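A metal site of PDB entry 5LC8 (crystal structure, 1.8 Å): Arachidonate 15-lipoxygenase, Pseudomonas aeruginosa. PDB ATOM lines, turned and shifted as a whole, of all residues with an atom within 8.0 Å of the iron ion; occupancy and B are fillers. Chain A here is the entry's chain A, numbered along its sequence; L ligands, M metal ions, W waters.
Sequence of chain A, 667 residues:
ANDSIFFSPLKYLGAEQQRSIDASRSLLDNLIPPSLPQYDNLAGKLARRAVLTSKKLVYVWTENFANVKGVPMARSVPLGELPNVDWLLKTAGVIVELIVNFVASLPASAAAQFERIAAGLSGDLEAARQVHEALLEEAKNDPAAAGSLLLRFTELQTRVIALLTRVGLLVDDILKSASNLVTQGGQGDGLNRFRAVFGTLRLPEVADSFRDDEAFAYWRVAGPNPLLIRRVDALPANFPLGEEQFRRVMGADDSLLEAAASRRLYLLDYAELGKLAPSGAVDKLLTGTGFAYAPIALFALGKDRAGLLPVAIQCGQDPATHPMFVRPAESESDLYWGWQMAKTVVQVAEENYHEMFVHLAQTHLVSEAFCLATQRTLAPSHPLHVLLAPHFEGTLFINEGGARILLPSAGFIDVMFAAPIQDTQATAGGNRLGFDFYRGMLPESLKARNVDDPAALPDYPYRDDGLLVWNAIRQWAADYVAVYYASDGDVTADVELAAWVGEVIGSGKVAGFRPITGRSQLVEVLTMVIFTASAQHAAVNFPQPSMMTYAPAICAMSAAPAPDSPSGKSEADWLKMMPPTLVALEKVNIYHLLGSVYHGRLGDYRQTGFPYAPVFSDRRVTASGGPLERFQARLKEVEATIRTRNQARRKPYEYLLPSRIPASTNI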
ATOM      1  N   GLU A 355      -9.545   3.566  35.631  1.00  0.00           N
ATOM      2  CA  GLU A 355     -10.241   2.860  34.550  1.00  0.00           C
ATOM      3  C   GLU A 355     -10.909   1.579  35.033  1.00  0.00           C
ATOM      4  O   GLU A 355     -12.056   1.310  34.684  1.00  0.00           O
ATOM      5  CB  GLU A 355      -9.327   2.619  33.348  1.00  0.00           C
ATOM      6  CG  GLU A 355      -8.993   3.885  32.584  1.00  0.00           C
ATOM      7  CD  GLU A 355     -10.163   4.446  31.787  1.00  0.00           C
ATOM      8  OE1 GLU A 355     -11.308   3.928  31.902  1.00  0.00           O
ATOM      9  OE2 GLU A 355      -9.941   5.438  31.037  1.00  0.00           O
ATOM     10  N   HIS A 359     -14.247   3.914  36.812  1.00  0.00           N
ATOM     11  CA  HIS A 359     -14.991   3.921  35.557  1.00  0.00           C
ATOM     12  C   HIS A 359     -15.693   2.576  35.304  1.00  0.00           C
ATOM     13  O   HIS A 359     -16.932   2.498  35.360  1.00  0.00           O
ATOM     14  CB  HIS A 359     -14.037   4.328  34.422  1.00  0.00           C
ATOM     15  CG  HIS A 359     -14.716   4.577  33.114  1.00  0.00           C
ATOM     16  ND1 HIS A 359     -14.036   4.590  31.925  1.00  0.00           N
ATOM     17  CD2 HIS A 359     -16.008   4.819  32.823  1.00  0.00           C
ATOM     18  CE1 HIS A 359     -14.886   4.826  30.942  1.00  0.00           C
ATOM     19  NE2 HIS A 359     -16.086   4.956  31.464  1.00  0.00           N
ATOM     20  N   LEU A 360     -14.943   1.504  35.068  1.00  0.00           N
ATOM     21  CA  LEU A 360     -15.559   0.229  34.662  1.00  0.00           C
ATOM     22  C   LEU A 360     -16.415  -0.373  35.764  1.00  0.00           C
ATOM     23  O   LEU A 360     -17.597  -0.643  35.561  1.00  0.00           O
ATOM     24  CB  LEU A 360     -14.499  -0.784  34.219  1.00  0.00           C
ATOM     25  CG  LEU A 360     -15.039  -2.189  33.873  1.00  0.00           C
ATOM     26  CD1 LEU A 360     -16.021  -2.143  32.683  1.00  0.00           C
ATOM     27  CD2 LEU A 360     -13.887  -3.135  33.584  1.00  0.00           C
ATOM     28  N   THR A 363     -19.322   2.512  37.654  1.00  0.00           N
ATOM     29  CA  THR A 363     -20.360   3.137  36.836  1.00  0.00           C
ATOM     30  C   THR A 363     -20.957   2.074  35.897  1.00  0.00           C
ATOM     31  O   THR A 363     -22.004   1.493  36.220  1.00  0.00           O
ATOM     32  CB  THR A 363     -19.869   4.417  36.084  1.00  0.00           C
ATOM     33  OG1 THR A 363     -18.878   4.104  35.120  1.00  0.00           O
ATOM     34  CG2 THR A 363     -19.306   5.454  37.078  1.00  0.00           C
ATOM     35  N   HIS A 364     -20.274   1.771  34.798  1.00  0.00           N
ATOM     36  CA  HIS A 364     -20.680   0.719  33.857  1.00  0.00           C
ATOM     37  C   HIS A 364     -21.267  -0.553  34.494  1.00  0.00           C
ATOM     38  O   HIS A 364     -22.401  -0.921  34.190  1.00  0.00           O
ATOM     39  CB  HIS A 364     -19.495   0.316  32.944  1.00  0.00           C
ATOM     40  CG  HIS A 364     -19.223   1.310  31.854  1.00  0.00           C
ATOM     41  ND1 HIS A 364     -19.788   1.212  30.611  1.00  0.00           N
ATOM     42  CD2 HIS A 364     -18.481   2.440  31.837  1.00  0.00           C
ATOM     43  CE1 HIS A 364     -19.387   2.221  29.855  1.00  0.00           C
ATOM     44  NE2 HIS A 364     -18.597   2.983  30.582  1.00  0.00           N
ATOM     45  N   ILE A 398     -23.175  -1.371  25.530  1.00  0.00           N
ATOM     46  CA  ILE A 398     -21.800  -0.897  25.707  1.00  0.00           C
ATOM     47  C   ILE A 398     -21.025  -1.835  26.628  1.00  0.00           C
ATOM     48  O   ILE A 398     -19.840  -2.042  26.421  1.00  0.00           O
ATOM     49  CB  ILE A 398     -21.713   0.588  26.164  1.00  0.00           C
ATOM     50  CG1 ILE A 398     -20.318   1.164  25.891  1.00  0.00           C
ATOM     51  CG2 ILE A 398     -22.057   0.761  27.639  1.00  0.00           C
ATOM     52  CD1 ILE A 398     -19.980   1.303  24.434  1.00  0.00           C
ATOM     53  N   ASN A 399     -21.694  -2.423  27.613  1.00  0.00           N
ATOM     54  CA  ASN A 399     -20.998  -3.325  28.533  1.00  0.00           C
ATOM     55  C   ASN A 399     -20.663  -4.686  27.901  1.00  0.00           C
ATOM     56  O   ASN A 399     -19.588  -5.246  28.153  1.00  0.00           O
ATOM     57  CB  ASN A 399     -21.779  -3.479  29.825  1.00  0.00           C
ATOM     58  CG  ASN A 399     -21.787  -2.207  30.658  1.00  0.00           C
ATOM     59  OD1 ASN A 399     -20.933  -1.324  30.481  1.00  0.00           O
ATOM     60  ND2 ASN A 399     -22.764  -2.096  31.554  1.00  0.00           N
ATOM     61  N   HIS A 537     -20.816   8.888  35.703  1.00  0.00           N
ATOM     62  CA  HIS A 537     -20.186   8.349  34.516  1.00  0.00           C
ATOM     63  C   HIS A 537     -19.570   9.460  33.668  1.00  0.00           C
ATOM     64  O   HIS A 537     -18.446   9.307  33.184  1.00  0.00           O
ATOM     65  CB  HIS A 537     -21.146   7.554  33.659  1.00  0.00           C
ATOM     66  CG  HIS A 537     -20.524   7.095  32.396  1.00  0.00           C
ATOM     67  ND1 HIS A 537     -20.801   7.656  31.184  1.00  0.00           N
ATOM     68  CD2 HIS A 537     -19.543   6.179  32.183  1.00  0.00           C
ATOM     69  CE1 HIS A 537     -20.066   7.076  30.249  1.00  0.00           C
ATOM     70  NE2 HIS A 537     -19.293   6.185  30.832  1.00  0.00           N
ATOM     71  N   ALA A 538     -20.297  10.562  33.493  1.00  0.00           N
ATOM     72  CA  ALA A 538     -19.787  11.689  32.719  1.00  0.00           C
ATOM     73  C   ALA A 538     -18.463  12.243  33.311  1.00  0.00           C
ATOM     74  O   ALA A 538     -17.500  12.473  32.593  1.00  0.00           O
ATOM     75  CB  ALA A 538     -20.828  12.800  32.635  1.00  0.00           C
ATOM     76  N   VAL A 540     -16.187  10.811  35.025  1.00  0.00           N
ATOM     77  CA  VAL A 540     -15.044   9.906  34.963  1.00  0.00           C
ATOM     78  C   VAL A 540     -14.746   9.407  33.529  1.00  0.00           C
ATOM     79  O   VAL A 540     -13.652   8.903  33.268  1.00  0.00           O
ATOM     80  CB  VAL A 540     -15.169   8.743  36.004  1.00  0.00           C
ATOM     81  CG1 VAL A 540     -15.466   9.308  37.395  1.00  0.00           C
ATOM     82  CG2 VAL A 540     -16.235   7.738  35.609  1.00  0.00           C
ATOM     83  N   ASN A 541     -15.692   9.604  32.602  1.00  0.00           N
ATOM     84  CA  ASN A 541     -15.557   9.145  31.223  1.00  0.00           C
ATOM     85  C   ASN A 541     -15.068  10.253  30.299  1.00  0.00           C
ATOM     86  O   ASN A 541     -14.131  10.056  29.531  1.00  0.00           O
ATOM     87  CB  ASN A 541     -16.887   8.564  30.742  1.00  0.00           C
ATOM     88  CG  ASN A 541     -16.851   8.069  29.304  1.00  0.00           C
ATOM     89  OD1 ASN A 541     -16.626   6.884  29.054  1.00  0.00           O
ATOM     90  ND2 ASN A 541     -17.072   8.976  28.354  1.00  0.00           N
ATOM     91  N   PHE A 542     -15.683  11.435  30.392  1.00  0.00           N
ATOM     92  CA  PHE A 542     -15.337  12.488  29.445  1.00  0.00           C
ATOM     93  C   PHE A 542     -13.991  13.207  29.634  1.00  0.00           C
ATOM     94  O   PHE A 542     -13.525  13.831  28.700  1.00  0.00           O
ATOM     95  CB  PHE A 542     -16.526  13.412  29.233  1.00  0.00           C
ATOM     96  CG  PHE A 542     -17.675  12.698  28.594  1.00  0.00           C
ATOM     97  CD1 PHE A 542     -17.599  12.295  27.274  1.00  0.00           C
ATOM     98  CD2 PHE A 542     -18.786  12.318  29.324  1.00  0.00           C
ATOM     99  CE1 PHE A 542     -18.622  11.578  26.674  1.00  0.00           C
ATOM    100  CE2 PHE A 542     -19.826  11.606  28.738  1.00  0.00           C
ATOM    101  CZ  PHE A 542     -19.741  11.232  27.410  1.00  0.00           C
ATOM    102  N   GLN A 544     -11.322  11.506  29.474  1.00  0.00           N
ATOM    103  CA  GLN A 544     -10.398  10.596  28.762  1.00  0.00           C
ATOM    104  C   GLN A 544      -9.658  11.247  27.572  1.00  0.00           C
ATOM    105  O   GLN A 544      -8.436  11.216  27.535  1.00  0.00           O
ATOM    106  CB  GLN A 544     -11.091   9.284  28.369  1.00  0.00           C
ATOM    107  CG  GLN A 544     -11.376   8.393  29.557  1.00  0.00           C
ATOM    108  CD  GLN A 544     -12.329   7.259  29.268  1.00  0.00           C
ATOM    109  OE1 GLN A 544     -13.469   7.479  28.800  1.00  0.00           O
ATOM    110  NE2 GLN A 544     -11.904   6.068  29.556  1.00  0.00           N
ATOM    111  N   LEU A 594     -13.965   6.882  23.388  1.00  0.00           N
ATOM    112  CA  LEU A 594     -14.849   6.730  24.544  1.00  0.00           C
ATOM    113  C   LEU A 594     -15.305   8.059  25.148  1.00  0.00           C
ATOM    114  O   LEU A 594     -16.354   8.107  25.783  1.00  0.00           O
ATOM    115  CB  LEU A 594     -14.192   5.875  25.625  1.00  0.00           C
ATOM    116  CG  LEU A 594     -13.850   4.436  25.212  1.00  0.00           C
ATOM    117  CD1 LEU A 594     -13.333   3.698  26.441  1.00  0.00           C
ATOM    118  CD2 LEU A 594     -15.021   3.713  24.578  1.00  0.00           C
ATOM    119  N   GLY A 595     -14.546   9.119  24.951  1.00  0.00           N
ATOM    120  CA  GLY A 595     -14.980  10.442  25.381  1.00  0.00           C
ATOM    121  C   GLY A 595     -15.504  11.345  24.279  1.00  0.00           C
ATOM    122  O   GLY A 595     -15.640  12.548  24.493  1.00  0.00           O
ATOM    123  N   SER A 664     -27.649   8.535  30.363  1.00  0.00           N
ATOM    124  CA  SER A 664     -27.249   7.158  30.615  1.00  0.00           C
ATOM    125  C   SER A 664     -25.760   6.926  30.325  1.00  0.00           C
ATOM    126  O   SER A 664     -25.061   7.787  29.771  1.00  0.00           O
ATOM    127  CB  SER A 664     -28.059   6.186  29.745  1.00  0.00           C
ATOM    128  OG  SER A 664     -27.660   6.242  28.370  1.00  0.00           O
ATOM    129  N   THR A 665     -25.299   5.749  30.725  1.00  0.00           N
ATOM    130  CA  THR A 665     -23.953   5.276  30.449  1.00  0.00           C
ATOM    131  C   THR A 665     -24.047   4.457  29.173  1.00  0.00           C
ATOM    132  O   THR A 665     -24.552   3.335  29.188  1.00  0.00           O
ATOM    133  CB  THR A 665     -23.452   4.437  31.644  1.00  0.00           C
ATOM    134  OG1 THR A 665     -23.371   5.295  32.787  1.00  0.00           O
ATOM    135  CG2 THR A 665     -22.106   3.807  31.389  1.00  0.00           C
ATOM    136  N   ASN A 666     -23.603   5.027  28.050  1.00  0.00           N
ATOM    137  CA  ASN A 666     -23.706   4.344  26.750  1.00  0.00           C
ATOM    138  C   ASN A 666     -22.425   4.381  25.919  1.00  0.00           C
ATOM    139  O   ASN A 666     -22.422   3.965  24.753  1.00  0.00           O
ATOM    140  CB  ASN A 666     -24.891   4.919  25.938  1.00  0.00           C
ATOM    141  CG  ASN A 666     -24.754   6.404  25.679  1.00  0.00           C
ATOM    142  OD1 ASN A 666     -23.872   6.834  24.927  1.00  0.00           O
ATOM    143  ND2 ASN A 666     -25.623   7.203  26.298  1.00  0.00           N
ATOM    144  N   ILE A 667     -21.336   4.848  26.516  1.00  0.00           N
ATOM    145  CA  ILE A 667     -20.039   4.867  25.855  1.00  0.00           C
ATOM    146  C   ILE A 667     -18.935   4.632  26.887  1.00  0.00           C
ATOM    147  O   ILE A 667     -19.111   4.894  28.100  1.00  0.00           O
ATOM    148  CB  ILE A 667     -19.803   6.187  25.104  1.00  0.00           C
ATOM    149  CG1 ILE A 667     -18.585   6.093  24.176  1.00  0.00           C
ATOM    150  CG2 ILE A 667     -19.632   7.350  26.079  1.00  0.00           C
ATOM    151  CD1 ILE A 667     -18.714   5.059  23.082  1.00  0.00           C
ATOM    152  OXT ILE A 667     -17.841   4.159  26.520  1.00  0.00           O
HETATM  153  N1  LIG L   1     -14.095  -7.662  16.333  1.00  0.00           N
HETATM  154  P1  LIG L   1     -18.286  -6.307  16.315  1.00  0.00           P
HETATM  155  C1  LIG L   1     -15.590  -2.008  16.613  1.00  0.00           C
HETATM  156  O1  LIG L   1     -15.545  -1.274  15.645  1.00  0.00           O
HETATM  157  C2  LIG L   1     -18.477  -3.827  15.568  1.00  0.00           C
HETATM  158  C3  LIG L   1     -17.936  -2.513  16.099  1.00  0.00           C
HETATM  159  O2  LIG L   1     -16.778  -2.791  16.880  1.00  0.00           O
HETATM  160  C4  LIG L   1     -19.024  -1.900  16.961  1.00  0.00           C
HETATM  161  O3  LIG L   1     -18.474  -0.962  17.879  1.00  0.00           O
HETATM  162  C5  LIG L   1     -15.782  -6.072  17.075  1.00  0.00           C
HETATM  163  C6  LIG L   1     -14.354  -6.239  16.600  1.00  0.00           C
HETATM  164  C7  LIG L   1     -19.337  -0.476  18.924  1.00  0.00           C
HETATM  165  O4  LIG L   1     -20.351  -1.086  19.182  1.00  0.00           O
HETATM  166  C8  LIG L   1     -14.404  -2.139  17.546  1.00  0.00           C
HETATM  167  C9  LIG L   1     -19.050   0.799  19.667  1.00  0.00           C
HETATM  168  O5  LIG L   1     -18.706  -7.140  17.483  1.00  0.00           O
HETATM  169  C10 LIG L   1     -13.875  -0.749  17.876  1.00  0.00           C
HETATM  170  C11 LIG L   1     -17.570   1.108  19.778  1.00  0.00           C
HETATM  171  O6  LIG L   1     -19.080  -6.661  15.079  1.00  0.00           O
HETATM  172  C12 LIG L   1     -12.649  -0.790  18.785  1.00  0.00           C
HETATM  173  C13 LIG L   1     -17.023   0.716  21.150  1.00  0.00           C
HETATM  174  O7  LIG L   1     -18.570  -4.760  16.637  1.00  0.00           O
HETATM  175  C14 LIG L   1     -12.125   0.615  19.066  1.00  0.00           C
HETATM  176  C15 LIG L   1     -16.339  -0.637  21.059  1.00  0.00           C
HETATM  177  O8  LIG L   1     -16.702  -6.466  16.049  1.00  0.00           O
HETATM  178  C16 LIG L   1     -11.272   1.084  17.908  1.00  0.00           C
HETATM  179  C17 LIG L   1     -15.524  -0.900  22.306  1.00  0.00           C
HETATM  180  C18 LIG L   1     -10.668   2.463  18.137  1.00  0.00           C
HETATM  181  C19 LIG L   1     -16.428  -1.105  23.509  1.00  0.00           C
HETATM  182  C20 LIG L   1     -10.472   3.229  16.834  1.00  0.00           C
HETATM  183  C21 LIG L   1     -16.375   0.098  24.449  1.00  0.00           C
HETATM  184  C22 LIG L   1      -9.729   2.442  15.746  1.00  0.00           C
HETATM  185  C23 LIG L   1     -16.687  -0.335  25.872  1.00  0.00           C
HETATM  186  C24 LIG L   1      -8.498   3.202  15.249  1.00  0.00           C
HETATM  187  C25 LIG L   1     -16.463   0.753  26.911  1.00  0.00           C
HETATM  188  C26 LIG L   1      -7.401   2.325  14.626  1.00  0.00           C
HETATM  189  C27 LIG L   1     -16.864   0.150  28.259  1.00  0.00           C
HETATM  190  C28 LIG L   1      -6.822   1.289  15.597  1.00  0.00           C
HETATM  191  C29 LIG L   1     -16.091   0.609  29.495  1.00  0.00           C
HETATM  192  C30 LIG L   1      -5.364   1.594  15.959  1.00  0.00           C
HETATM  193  C31 LIG L   1     -14.610   0.281  29.491  1.00  0.00           C
HETATM  194  C32 LIG L   1      -4.798   0.516  16.865  1.00  0.00           C
HETATM  195  C33 LIG L   1     -13.881   1.237  30.428  1.00  0.00           C
HETATM  196  C34 LIG L   1     -12.413   0.883  30.527  1.00  0.00           C
HETATM  197  C35 LIG L   1     -11.659   1.282  29.272  1.00  0.00           C
HETATM  198  C36 LIG L   1     -10.167   1.035  29.449  1.00  0.00           C
HETATM  199  C37 LIG L   1      -9.442   0.957  28.123  1.00  0.00           C
HETATM  200 FE    FE M   1     -17.737   4.974  29.856  1.00  0.00          FE
HETATM  201  O   HOH W   1     -16.315   3.846  28.532  1.00  0.00           O
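A ring nitrogen (NE2) of His 537 is bound to the iron ion (2.2 Å). The iron ion is bound by O of Ile 667 (2.2 Å). The iron ion is bound by water W1, 2.2 Å away. NE2 of His 364 is bound to the iron ion. A ring nitrogen (NE2) of His 359 is bound to the iron ion, 2.3 Å away. The side-chain amide oxygen (OD1) of Asn 541 is bound to the iron ion (2.4 Å). The iron ion has six donor atoms within binding distance.
A ring nitrogen (ND1) of His 364 lies within hydrogen-bond range of the side-chain amide oxygen (OD1) of Asn 399. The backbone carbonyl oxygen of His 359 lies within hydrogen-bond range of the side-chain hydroxyl of Thr 363, 2.5 Å away. The side-chain carboxylate (OE1) of Glu 355 lies within hydrogen-bond range of a ring nitrogen (ND1) of His 359 (2.8 Å). The backbone carbonyl oxygen (O) of Asn 541 lies close to the side-chain amide oxygen (OE1) of Gln 544. O of Leu 594 lies within hydrogen-bond range of ND2 of Asn 541, at 2.8 Å.
Within 4 Å of the iron ion: His 359, His 364, His 537, Asn 541 and Ile 667.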
